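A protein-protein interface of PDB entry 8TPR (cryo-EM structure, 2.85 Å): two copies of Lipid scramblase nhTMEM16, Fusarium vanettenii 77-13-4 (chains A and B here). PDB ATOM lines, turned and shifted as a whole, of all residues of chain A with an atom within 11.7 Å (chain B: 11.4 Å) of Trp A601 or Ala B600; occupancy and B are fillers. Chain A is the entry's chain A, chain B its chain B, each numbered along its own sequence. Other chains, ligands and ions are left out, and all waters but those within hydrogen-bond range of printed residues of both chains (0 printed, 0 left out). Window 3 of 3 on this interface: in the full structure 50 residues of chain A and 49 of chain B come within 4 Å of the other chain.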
ATOM      1  N   TYR A 219     -43.366  -9.873  16.371  1.00  0.00           N
ATOM      2  CA  TYR A 219     -42.405  -9.865  15.274  1.00  0.00           C
ATOM      3  C   TYR A 219     -42.960 -10.562  14.040  1.00  0.00           C
ATOM      4  O   TYR A 219     -42.772 -10.085  12.911  1.00  0.00           O
ATOM      5  CB  TYR A 219     -41.104 -10.530  15.724  1.00  0.00           C
ATOM      6  CG  TYR A 219     -39.899 -10.161  14.894  1.00  0.00           C
ATOM      7  CD1 TYR A 219     -39.686 -10.739  13.650  1.00  0.00           C
ATOM      8  CD2 TYR A 219     -38.972  -9.240  15.355  1.00  0.00           C
ATOM      9  CE1 TYR A 219     -38.586 -10.406  12.888  1.00  0.00           C
ATOM     10  CE2 TYR A 219     -37.868  -8.901  14.599  1.00  0.00           C
ATOM     11  CZ  TYR A 219     -37.681  -9.487  13.366  1.00  0.00           C
ATOM     12  OH  TYR A 219     -36.584  -9.156  12.608  1.00  0.00           O
ATOM     13  N   SER A 578     -39.974  -3.929  12.331  1.00  0.00           N
ATOM     14  CA  SER A 578     -39.178  -4.822  13.162  1.00  0.00           C
ATOM     15  C   SER A 578     -38.387  -4.051  14.206  1.00  0.00           C
ATOM     16  O   SER A 578     -38.294  -4.480  15.362  1.00  0.00           O
ATOM     17  CB  SER A 578     -38.245  -5.658  12.291  1.00  0.00           C
ATOM     18  OG  SER A 578     -38.984  -6.612  11.552  1.00  0.00           O
ATOM     19  N   ALA A 579     -37.827  -2.901  13.826  1.00  0.00           N
ATOM     20  CA  ALA A 579     -37.114  -2.082  14.799  1.00  0.00           C
ATOM     21  C   ALA A 579     -38.012  -1.753  15.980  1.00  0.00           C
ATOM     22  O   ALA A 579     -37.624  -1.931  17.141  1.00  0.00           O
ATOM     23  CB  ALA A 579     -36.597  -0.806  14.138  1.00  0.00           C
ATOM     24  N   TYR A 582     -38.321  -4.570  18.289  1.00  0.00           N
ATOM     25  CA  TYR A 582     -37.197  -4.742  19.197  1.00  0.00           C
ATOM     26  C   TYR A 582     -37.158  -3.662  20.266  1.00  0.00           C
ATOM     27  O   TYR A 582     -36.761  -3.938  21.402  1.00  0.00           O
ATOM     28  CB  TYR A 582     -35.879  -4.753  18.427  1.00  0.00           C
ATOM     29  CG  TYR A 582     -34.696  -5.088  19.303  1.00  0.00           C
ATOM     30  CD1 TYR A 582     -34.416  -6.402  19.648  1.00  0.00           C
ATOM     31  CD2 TYR A 582     -33.874  -4.091  19.804  1.00  0.00           C
ATOM     32  CE1 TYR A 582     -33.341  -6.712  20.453  1.00  0.00           C
ATOM     33  CE2 TYR A 582     -32.797  -4.393  20.611  1.00  0.00           C
ATOM     34  CZ  TYR A 582     -32.537  -5.705  20.932  1.00  0.00           C
ATOM     35  OH  TYR A 582     -31.465  -6.013  21.736  1.00  0.00           O
ATOM     36  N   LEU A 583     -37.564  -2.439  19.933  1.00  0.00           N
ATOM     37  CA  LEU A 583     -37.364  -1.322  20.845  1.00  0.00           C
ATOM     38  C   LEU A 583     -38.474  -1.179  21.874  1.00  0.00           C
ATOM     39  O   LEU A 583     -38.305  -0.433  22.843  1.00  0.00           O
ATOM     40  CB  LEU A 583     -37.229  -0.020  20.054  1.00  0.00           C
ATOM     41  CG  LEU A 583     -35.906   0.137  19.306  1.00  0.00           C
ATOM     42  CD1 LEU A 583     -35.952   1.332  18.376  1.00  0.00           C
ATOM     43  CD2 LEU A 583     -34.761   0.268  20.287  1.00  0.00           C
ATOM     44  N   ASN A 586     -38.601  -4.720  24.898  1.00  0.00           N
ATOM     45  CA  ASN A 586     -37.632  -4.753  25.988  1.00  0.00           C
ATOM     46  C   ASN A 586     -37.129  -3.353  26.327  1.00  0.00           C
ATOM     47  O   ASN A 586     -37.511  -2.374  25.687  1.00  0.00           O
ATOM     48  CB  ASN A 586     -36.455  -5.659  25.628  1.00  0.00           C
ATOM     49  CG  ASN A 586     -35.894  -5.366  24.254  1.00  0.00           C
ATOM     50  OD1 ASN A 586     -35.160  -4.396  24.065  1.00  0.00           O
ATOM     51  ND2 ASN A 586     -36.238  -6.203  23.284  1.00  0.00           N
ATOM     52  N   LYS A 599     -29.402  -3.435  23.892  1.00  0.00           N
ATOM     53  CA  LYS A 599     -28.276  -3.961  23.131  1.00  0.00           C
ATOM     54  C   LYS A 599     -28.438  -3.666  21.646  1.00  0.00           C
ATOM     55  O   LYS A 599     -29.388  -4.123  21.015  1.00  0.00           O
ATOM     56  CB  LYS A 599     -28.133  -5.466  23.356  1.00  0.00           C
ATOM     57  N   ALA A 600     -27.500  -2.894  21.092  1.00  0.00           N
ATOM     58  CA  ALA A 600     -27.574  -2.529  19.684  1.00  0.00           C
ATOM     59  C   ALA A 600     -27.397  -3.727  18.760  1.00  0.00           C
ATOM     60  O   ALA A 600     -27.886  -3.693  17.625  1.00  0.00           O
ATOM     61  CB  ALA A 600     -26.526  -1.467  19.359  1.00  0.00           C
ATOM     62  N   TRP A 601     -26.711  -4.776  19.219  1.00  0.00           N
ATOM     63  CA  TRP A 601     -26.510  -5.949  18.375  1.00  0.00           C
ATOM     64  C   TRP A 601     -27.837  -6.591  18.001  1.00  0.00           C
ATOM     65  O   TRP A 601     -28.056  -6.948  16.838  1.00  0.00           O
ATOM     66  CB  TRP A 601     -25.607  -6.957  19.088  1.00  0.00           C
ATOM     67  CG  TRP A 601     -25.892  -8.377  18.719  1.00  0.00           C
ATOM     68  CD1 TRP A 601     -25.649  -8.977  17.520  1.00  0.00           C
ATOM     69  CD2 TRP A 601     -26.478  -9.380  19.558  1.00  0.00           C
ATOM     70  NE1 TRP A 601     -26.046 -10.290  17.558  1.00  0.00           N
ATOM     71  CE2 TRP A 601     -26.560 -10.562  18.798  1.00  0.00           C
ATOM     72  CE3 TRP A 601     -26.942  -9.391  20.876  1.00  0.00           C
ATOM     73  CZ2 TRP A 601     -27.085 -11.744  19.311  1.00  0.00           C
ATOM     74  CZ3 TRP A 601     -27.464 -10.566  21.384  1.00  0.00           C
ATOM     75  CH2 TRP A 601     -27.531 -11.727  20.604  1.00  0.00           C
ATOM     76  N   GLY A 602     -28.741  -6.737  18.971  1.00  0.00           N
ATOM     77  CA  GLY A 602     -30.034  -7.330  18.676  1.00  0.00           C
ATOM     78  C   GLY A 602     -30.861  -6.486  17.727  1.00  0.00           C
ATOM     79  O   GLY A 602     -31.512  -7.010  16.822  1.00  0.00           O
ATOM     80  N   LEU A 603     -30.848  -5.166  17.921  1.00  0.00           N
ATOM     81  CA  LEU A 603     -31.600  -4.280  17.040  1.00  0.00           C
ATOM     82  C   LEU A 603     -31.070  -4.351  15.614  1.00  0.00           C
ATOM     83  O   LEU A 603     -31.846  -4.442  14.654  1.00  0.00           O
ATOM     84  CB  LEU A 603     -31.538  -2.848  17.567  1.00  0.00           C
ATOM     85  CG  LEU A 603     -31.884  -1.741  16.574  1.00  0.00           C
ATOM     86  CD1 LEU A 603     -33.378  -1.696  16.337  1.00  0.00           C
ATOM     87  CD2 LEU A 603     -31.383  -0.404  17.078  1.00  0.00           C
ATOM     88  N   LEU A 604     -29.746  -4.319  15.459  1.00  0.00           N
ATOM     89  CA  LEU A 604     -29.165  -4.405  14.125  1.00  0.00           C
ATOM     90  C   LEU A 604     -29.450  -5.755  13.485  1.00  0.00           C
ATOM     91  O   LEU A 604     -29.724  -5.829  12.282  1.00  0.00           O
ATOM     92  CB  LEU A 604     -27.662  -4.144  14.186  1.00  0.00           C
ATOM     93  CG  LEU A 604     -27.263  -2.726  14.583  1.00  0.00           C
ATOM     94  CD1 LEU A 604     -25.759  -2.591  14.607  1.00  0.00           C
ATOM     95  CD2 LEU A 604     -27.875  -1.722  13.629  1.00  0.00           C
ATOM     96  N   LEU A 605     -29.394  -6.836  14.265  1.00  0.00           N
ATOM     97  CA  LEU A 605     -29.692  -8.154  13.716  1.00  0.00           C
ATOM     98  C   LEU A 605     -31.143  -8.249  13.266  1.00  0.00           C
ATOM     99  O   LEU A 605     -31.436  -8.809  12.204  1.00  0.00           O
ATOM    100  CB  LEU A 605     -29.378  -9.235  14.746  1.00  0.00           C
ATOM    101  CG  LEU A 605     -29.379 -10.672  14.231  1.00  0.00           C
ATOM    102  CD1 LEU A 605     -28.588 -10.777  12.942  1.00  0.00           C
ATOM    103  CD2 LEU A 605     -28.819 -11.608  15.282  1.00  0.00           C
ATOM    104  N   SER A 606     -32.068  -7.706  14.062  1.00  0.00           N
ATOM    105  CA  SER A 606     -33.475  -7.729  13.677  1.00  0.00           C
ATOM    106  C   SER A 606     -33.715  -6.907  12.419  1.00  0.00           C
ATOM    107  O   SER A 606     -34.448  -7.335  11.521  1.00  0.00           O
ATOM    108  CB  SER A 606     -34.342  -7.221  14.824  1.00  0.00           C
ATOM    109  OG  SER A 606     -34.177  -5.827  14.997  1.00  0.00           O
ATOM    110  N   ILE A 607     -33.099  -5.726  12.332  1.00  0.00           N
ATOM    111  CA  ILE A 607     -33.250  -4.897  11.139  1.00  0.00           C
ATOM    112  C   ILE A 607     -32.691  -5.614   9.917  1.00  0.00           C
ATOM    113  O   ILE A 607     -33.312  -5.625   8.847  1.00  0.00           O
ATOM    114  CB  ILE A 607     -32.572  -3.530  11.351  1.00  0.00           C
ATOM    115  CG1 ILE A 607     -33.427  -2.648  12.257  1.00  0.00           C
ATOM    116  CG2 ILE A 607     -32.327  -2.841  10.024  1.00  0.00           C
ATOM    117  CD1 ILE A 607     -32.779  -1.332  12.601  1.00  0.00           C
ATOM    118  N   LEU A 608     -31.513  -6.223  10.058  1.00  0.00           N
ATOM    119  CA  LEU A 608     -30.898  -6.947   8.950  1.00  0.00           C
ATOM    120  C   LEU A 608     -31.784  -8.093   8.484  1.00  0.00           C
ATOM    121  O   LEU A 608     -32.031  -8.256   7.282  1.00  0.00           O
ATOM    122  CB  LEU A 608     -29.530  -7.472   9.384  1.00  0.00           C
ATOM    123  CG  LEU A 608     -28.438  -7.637   8.330  1.00  0.00           C
ATOM    124  CD1 LEU A 608     -28.412  -6.446   7.402  1.00  0.00           C
ATOM    125  CD2 LEU A 608     -27.091  -7.825   9.000  1.00  0.00           C
ATOM    126  N   PHE A 609     -32.275  -8.900   9.427  1.00  0.00           N
ATOM    127  CA  PHE A 609     -33.114 -10.032   9.059  1.00  0.00           C
ATOM    128  C   PHE A 609     -34.397  -9.569   8.389  1.00  0.00           C
ATOM    129  O   PHE A 609     -34.817 -10.147   7.384  1.00  0.00           O
ATOM    130  CB  PHE A 609     -33.438 -10.884  10.283  1.00  0.00           C
ATOM    131  CG  PHE A 609     -34.485 -11.928  10.024  1.00  0.00           C
ATOM    132  CD1 PHE A 609     -34.212 -13.015   9.213  1.00  0.00           C
ATOM    133  CD2 PHE A 609     -35.749 -11.816  10.577  1.00  0.00           C
ATOM    134  CE1 PHE A 609     -35.172 -13.974   8.967  1.00  0.00           C
ATOM    135  CE2 PHE A 609     -36.714 -12.772  10.332  1.00  0.00           C
ATOM    136  CZ  PHE A 609     -36.425 -13.852   9.527  1.00  0.00           C
ATOM    137  N   ALA A 610     -35.031  -8.525   8.923  1.00  0.00           N
ATOM    138  CA  ALA A 610     -36.280  -8.048   8.341  1.00  0.00           C
ATOM    139  C   ALA A 610     -36.063  -7.509   6.934  1.00  0.00           C
ATOM    140  O   ALA A 610     -36.832  -7.814   6.017  1.00  0.00           O
ATOM    141  CB  ALA A 610     -36.896  -6.977   9.236  1.00  0.00           C
ATOM    142  N   PRO B 396     -12.995 -15.255  12.985  1.00  0.00           N
ATOM    143  CA  PRO B 396     -13.877 -14.901  14.106  1.00  0.00           C
ATOM    144  C   PRO B 396     -13.897 -15.963  15.191  1.00  0.00           C
ATOM    145  O   PRO B 396     -13.804 -15.646  16.380  1.00  0.00           O
ATOM    146  CB  PRO B 396     -15.254 -14.757  13.442  1.00  0.00           C
ATOM    147  CG  PRO B 396     -14.968 -14.562  12.002  1.00  0.00           C
ATOM    148  CD  PRO B 396     -13.759 -15.389  11.734  1.00  0.00           C
ATOM    149  N   PHE B 397     -14.018 -17.225  14.793  1.00  0.00           N
ATOM    150  CA  PHE B 397     -14.100 -18.348  15.723  1.00  0.00           C
ATOM    151  C   PHE B 397     -12.801 -19.142  15.602  1.00  0.00           C
ATOM    152  O   PHE B 397     -12.707 -20.094  14.827  1.00  0.00           O
ATOM    153  CB  PHE B 397     -15.320 -19.226  15.437  1.00  0.00           C
ATOM    154  CG  PHE B 397     -16.552 -18.458  15.045  1.00  0.00           C
ATOM    155  CD1 PHE B 397     -16.894 -17.279  15.685  1.00  0.00           C
ATOM    156  CD2 PHE B 397     -17.373 -18.924  14.034  1.00  0.00           C
ATOM    157  CE1 PHE B 397     -18.024 -16.580  15.319  1.00  0.00           C
ATOM    158  CE2 PHE B 397     -18.506 -18.227  13.666  1.00  0.00           C
ATOM    159  CZ  PHE B 397     -18.832 -17.055  14.309  1.00  0.00           C
ATOM    160  N   SER B 578     -16.564  -5.378   3.373  1.00  0.00           N
ATOM    161  CA  SER B 578     -16.583  -4.594   4.602  1.00  0.00           C
ATOM    162  C   SER B 578     -16.505  -5.489   5.828  1.00  0.00           C
ATOM    163  O   SER B 578     -15.795  -5.169   6.789  1.00  0.00           O
ATOM    164  CB  SER B 578     -17.834  -3.725   4.651  1.00  0.00           C
ATOM    165  OG  SER B 578     -17.744  -2.679   3.702  1.00  0.00           O
ATOM    166  N   ALA B 579     -17.208  -6.622   5.809  1.00  0.00           N
ATOM    167  CA  ALA B 579     -17.121  -7.554   6.927  1.00  0.00           C
ATOM    168  C   ALA B 579     -15.676  -7.950   7.179  1.00  0.00           C
ATOM    169  O   ALA B 579     -15.191  -7.893   8.315  1.00  0.00           O
ATOM    170  CB  ALA B 579     -17.983  -8.786   6.658  1.00  0.00           C
ATOM    171  N   TYR B 582     -13.833  -5.341   8.957  1.00  0.00           N
ATOM    172  CA  TYR B 582     -14.067  -5.297  10.392  1.00  0.00           C
ATOM    173  C   TYR B 582     -13.418  -6.470  11.111  1.00  0.00           C
ATOM    174  O   TYR B 582     -12.955  -6.313  12.244  1.00  0.00           O
ATOM    175  CB  TYR B 582     -15.563  -5.272  10.694  1.00  0.00           C
ATOM    176  CG  TYR B 582     -15.858  -5.065  12.159  1.00  0.00           C
ATOM    177  CD1 TYR B 582     -15.802  -3.800  12.725  1.00  0.00           C
ATOM    178  CD2 TYR B 582     -16.169  -6.136  12.983  1.00  0.00           C
ATOM    179  CE1 TYR B 582     -16.063  -3.609  14.065  1.00  0.00           C
ATOM    180  CE2 TYR B 582     -16.433  -5.953  14.324  1.00  0.00           C
ATOM    181  CZ  TYR B 582     -16.376  -4.687  14.859  1.00  0.00           C
ATOM    182  OH  TYR B 582     -16.637  -4.496  16.195  1.00  0.00           O
ATOM    183  N   LEU B 583     -13.372  -7.640  10.479  1.00  0.00           N
ATOM    184  CA  LEU B 583     -12.948  -8.841  11.184  1.00  0.00           C
ATOM    185  C   LEU B 583     -11.440  -9.030  11.200  1.00  0.00           C
ATOM    186  O   LEU B 583     -10.945  -9.867  11.962  1.00  0.00           O
ATOM    187  CB  LEU B 583     -13.610 -10.072  10.562  1.00  0.00           C
ATOM    188  CG  LEU B 583     -15.101 -10.215  10.867  1.00  0.00           C
ATOM    189  CD1 LEU B 583     -15.717 -11.319  10.033  1.00  0.00           C
ATOM    190  CD2 LEU B 583     -15.311 -10.481  12.343  1.00  0.00           C
ATOM    191  N   ASN B 586      -9.239  -5.772  13.698  1.00  0.00           N
ATOM    192  CA  ASN B 586      -9.240  -5.877  15.153  1.00  0.00           C
ATOM    193  C   ASN B 586      -9.432  -7.321  15.606  1.00  0.00           C
ATOM    194  O   ASN B 586      -9.599  -8.223  14.786  1.00  0.00           O
ATOM    195  CB  ASN B 586     -10.333  -4.992  15.751  1.00  0.00           C
ATOM    196  CG  ASN B 586     -11.672  -5.183  15.073  1.00  0.00           C
ATOM    197  OD1 ASN B 586     -12.374  -6.162  15.327  1.00  0.00           O
ATOM    198  ND2 ASN B 586     -12.034  -4.249  14.203  1.00  0.00           N
ATOM    199  N   LYS B 599     -16.825  -7.340  18.921  1.00  0.00           N
ATOM    200  CA  LYS B 599     -18.157  -6.794  19.151  1.00  0.00           C
ATOM    201  C   LYS B 599     -19.028  -6.949  17.912  1.00  0.00           C
ATOM    202  O   LYS B 599     -18.723  -6.398  16.856  1.00  0.00           O
ATOM    203  CB  LYS B 599     -18.072  -5.322  19.555  1.00  0.00           C
ATOM    204  N   ALA B 600     -20.119  -7.705  18.047  1.00  0.00           N
ATOM    205  CA  ALA B 600     -21.008  -7.940  16.917  1.00  0.00           C
ATOM    206  C   ALA B 600     -21.718  -6.672  16.461  1.00  0.00           C
ATOM    207  O   ALA B 600     -22.106  -6.584  15.290  1.00  0.00           O
ATOM    208  CB  ALA B 600     -22.038  -9.010  17.270  1.00  0.00           C
ATOM    209  N   TRP B 601     -21.897  -5.698  17.355  1.00  0.00           N
ATOM    210  CA  TRP B 601     -22.573  -4.462  16.972  1.00  0.00           C
ATOM    211  C   TRP B 601     -21.810  -3.736  15.876  1.00  0.00           C
ATOM    212  O   TRP B 601     -22.407  -3.267  14.900  1.00  0.00           O
ATOM    213  CB  TRP B 601     -22.747  -3.561  18.195  1.00  0.00           C
ATOM    214  CG  TRP B 601     -22.738  -2.102  17.865  1.00  0.00           C
ATOM    215  CD1 TRP B 601     -23.698  -1.408  17.191  1.00  0.00           C
ATOM    216  CD2 TRP B 601     -21.715  -1.156  18.196  1.00  0.00           C
ATOM    217  NE1 TRP B 601     -23.338  -0.089  17.081  1.00  0.00           N
ATOM    218  CE2 TRP B 601     -22.124   0.093  17.689  1.00  0.00           C
ATOM    219  CE3 TRP B 601     -20.494  -1.244  18.869  1.00  0.00           C
ATOM    220  CZ2 TRP B 601     -21.357   1.244  17.833  1.00  0.00           C
ATOM    221  CZ3 TRP B 601     -19.732  -0.099  19.012  1.00  0.00           C
ATOM    222  CH2 TRP B 601     -20.166   1.129  18.498  1.00  0.00           C
ATOM    223  N   GLY B 602     -20.487  -3.640  16.012  1.00  0.00           N
ATOM    224  CA  GLY B 602     -19.697  -2.970  14.992  1.00  0.00           C
ATOM    225  C   GLY B 602     -19.732  -3.691  13.660  1.00  0.00           C
ATOM    226  O   GLY B 602     -19.830  -3.062  12.605  1.00  0.00           O
ATOM    227  N   LEU B 603     -19.651  -5.023  13.688  1.00  0.00           N
ATOM    228  CA  LEU B 603     -19.698  -5.794  12.451  1.00  0.00           C
ATOM    229  C   LEU B 603     -21.037  -5.618  11.749  1.00  0.00           C
ATOM    230  O   LEU B 603     -21.092  -5.410  10.529  1.00  0.00           O
ATOM    231  CB  LEU B 603     -19.436  -7.270  12.748  1.00  0.00           C
ATOM    232  CG  LEU B 603     -19.867  -8.267  11.677  1.00  0.00           C
ATOM    233  CD1 LEU B 603     -18.908  -8.230  10.507  1.00  0.00           C
ATOM    234  CD2 LEU B 603     -19.945  -9.664  12.258  1.00  0.00           C
ATOM    235  N   LEU B 604     -22.132  -5.690  12.507  1.00  0.00           N
ATOM    236  CA  LEU B 604     -23.448  -5.509  11.909  1.00  0.00           C
ATOM    237  C   LEU B 604     -23.620  -4.096  11.371  1.00  0.00           C
ATOM    238  O   LEU B 604     -24.210  -3.904  10.303  1.00  0.00           O
ATOM    239  CB  LEU B 604     -24.541  -5.836  12.924  1.00  0.00           C
ATOM    240  CG  LEU B 604     -24.617  -7.300  13.351  1.00  0.00           C
ATOM    241  CD1 LEU B 604     -25.730  -7.498  14.350  1.00  0.00           C
ATOM    242  CD2 LEU B 604     -24.820  -8.187  12.140  1.00  0.00           C
ATOM    243  N   LEU B 605     -23.114  -3.092  12.091  1.00  0.00           N
ATOM    244  CA  LEU B 605     -23.218  -1.720  11.609  1.00  0.00           C
ATOM    245  C   LEU B 605     -22.427  -1.526  10.322  1.00  0.00           C
ATOM    246  O   LEU B 605     -22.896  -0.861   9.393  1.00  0.00           O
ATOM    247  CB  LEU B 605     -22.738  -0.750  12.685  1.00  0.00           C
ATOM    248  CG  LEU B 605     -23.038   0.727  12.438  1.00  0.00           C
ATOM    249  CD1 LEU B 605     -24.482   0.914  12.012  1.00  0.00           C
ATOM    250  CD2 LEU B 605     -22.734   1.542  13.678  1.00  0.00           C
ATOM    251  N   SER B 606     -21.223  -2.099  10.251  1.00  0.00           N
ATOM    252  CA  SER B 606     -20.425  -1.983   9.035  1.00  0.00           C
ATOM    253  C   SER B 606     -21.103  -2.679   7.863  1.00  0.00           C
ATOM    254  O   SER B 606     -21.137  -2.143   6.751  1.00  0.00           O
ATOM    255  CB  SER B 606     -19.031  -2.556   9.266  1.00  0.00           C
ATOM    256  OG  SER B 606     -19.079  -3.966   9.372  1.00  0.00           O
ATOM    257  N   ILE B 607     -21.655  -3.872   8.095  1.00  0.00           N
ATOM    258  CA  ILE B 607     -22.357  -4.584   7.030  1.00  0.00           C
ATOM    259  C   ILE B 607     -23.565  -3.784   6.559  1.00  0.00           C
ATOM    260  O   ILE B 607     -23.809  -3.651   5.354  1.00  0.00           O
ATOM    261  CB  ILE B 607     -22.762  -5.991   7.508  1.00  0.00           C
ATOM    262  CG1 ILE B 607     -21.548  -6.914   7.532  1.00  0.00           C
ATOM    263  CG2 ILE B 607     -23.845  -6.567   6.619  1.00  0.00           C
ATOM    264  CD1 ILE B 607     -21.843  -8.282   8.093  1.00  0.00           C
ATOM    265  N   LEU B 608     -24.335  -3.239   7.502  1.00  0.00           N
ATOM    266  CA  LEU B 608     -25.508  -2.445   7.154  1.00  0.00           C
ATOM    267  C   LEU B 608     -25.122  -1.226   6.328  1.00  0.00           C
ATOM    268  O   LEU B 608     -25.729  -0.946   5.286  1.00  0.00           O
ATOM    269  CB  LEU B 608     -26.230  -2.017   8.432  1.00  0.00           C
ATOM    270  CG  LEU B 608     -27.740  -1.803   8.387  1.00  0.00           C
ATOM    271  CD1 LEU B 608     -28.409  -2.906   7.602  1.00  0.00           C
ATOM    272  CD2 LEU B 608     -28.299  -1.732   9.795  1.00  0.00           C
ATOM    273  N   PHE B 609     -24.107  -0.487   6.781  1.00  0.00           N
ATOM    274  CA  PHE B 609     -23.691   0.708   6.058  1.00  0.00           C
ATOM    275  C   PHE B 609     -23.188   0.360   4.667  1.00  0.00           C
ATOM    276  O   PHE B 609     -23.522   1.043   3.696  1.00  0.00           O
ATOM    277  CB  PHE B 609     -22.612   1.459   6.835  1.00  0.00           C
ATOM    278  CG  PHE B 609     -21.970   2.563   6.047  1.00  0.00           C
ATOM    279  CD1 PHE B 609     -22.681   3.708   5.728  1.00  0.00           C
ATOM    280  CD2 PHE B 609     -20.661   2.455   5.610  1.00  0.00           C
ATOM    281  CE1 PHE B 609     -22.098   4.724   4.999  1.00  0.00           C
ATOM    282  CE2 PHE B 609     -20.074   3.469   4.880  1.00  0.00           C
ATOM    283  CZ  PHE B 609     -20.793   4.604   4.574  1.00  0.00           C
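Of the 18 printed residues of chain B, 5 touch a printed residue of chain A.
Hydrophobic or aromatic side chains of chain B within 4 Å of the printed part of chain A: Ala B600, Trp B601, Leu B604 and Leu B608.
Printed residues of chain A that touch a printed residue of chain B: Ala A600, Trp A601, Leu A604, Leu A605 and Leu A608.
Along chain A the printed residues that touch a printed residue of chain B span positions 600 to 608.
Among the printed residues, 10 pairs touch across the chains.
Among the printed residues, no Asp or Glu carboxylate lies within 4 Å of a Lys or Arg side-chain nitrogen of the other chain.
Of chain B, only Ala B600 (3.6 Å) and Leu B604 (3.5 Å) come within 4 Å of Trp A601.
No residue of chain B comes within 4 Å of Gly A602.
Leu A604 touches just these residues of chain B: Trp B601, Leu B604, Leu B605 and Leu B608.
Of the printed residues of chain B, Leu A608 touches Leu B604 and Leu B608.
Pro B396 touches none of the printed residues of chain A.
Lys B599 touches none of the printed residues of chain A.
Ala B600 touches just one residue of chain A: Trp A601.
Printed residues of chain A within 4 Å of Trp B601: Ala A600 (3.6 Å) and Leu A604 (3.4 Å).
No residue of chain A comes within 4 Å of Leu B603.
Printed residues of chain A within 4 Å of Leu B605: Leu A604.
Of the printed residues of chain A, Leu B608 touches Leu A604 (3.9 Å) and Leu A608 (3.5 Å).
The nearest residue of chain B that does not touch Trp A601 is Trp B601 (4.3 Å).
The nearest residue of chain A that does not touch Ala B600 is Leu A604 (5.5 Å).
The nearest printed residue of chain A that does not touch Leu B605 is Leu A608 (6.9 Å).
CB of Ala A600 touches CD1 of Trp B601, 3.6 Å away.
CD1 of Trp A601 touches CB of Ala B600 (3.6 Å).
Trp A601 touches Leu B604.
Trp B601 touches Leu A604 (O to CD1, 3.4 Å).
CB of Leu A604 touches CB of Leu B604, at 3.8 Å.
Leu B605 touches Leu A604 (N to CD1, 3.7 Å).
CD2 of Leu B608 touches CD2 of Leu A604, 3.9 Å away.
Leu A605 touches Leu B604 (N to CD1, 3.7 Å).
CD2 of Leu B604 touches CD2 of Leu A608 (3.9 Å).
Leu A608 touches Leu B608 (CD1 to CD1, 3.5 Å).
Trp A601 touches Leu B604, and with the chains exchanged Leu A604 touches Trp B601.
Leu A604 touches Leu B605, and with the chains exchanged Leu A605 touches Leu B604.
Leu A604 touches Leu B608, and with the chains exchanged Leu A608 touches Leu B604.
Leu A608 touches its own counterpart, Leu B608.
Positions printed for both chains: 578, 579, 582, 583, 586, 599, 600, 601, 602, 603, 604, 605, 606, 607, 608 and 609.
Of the 10 pairs that touch across the chains among the printed residues, 10 have their exchanged pair printed and touching as well.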
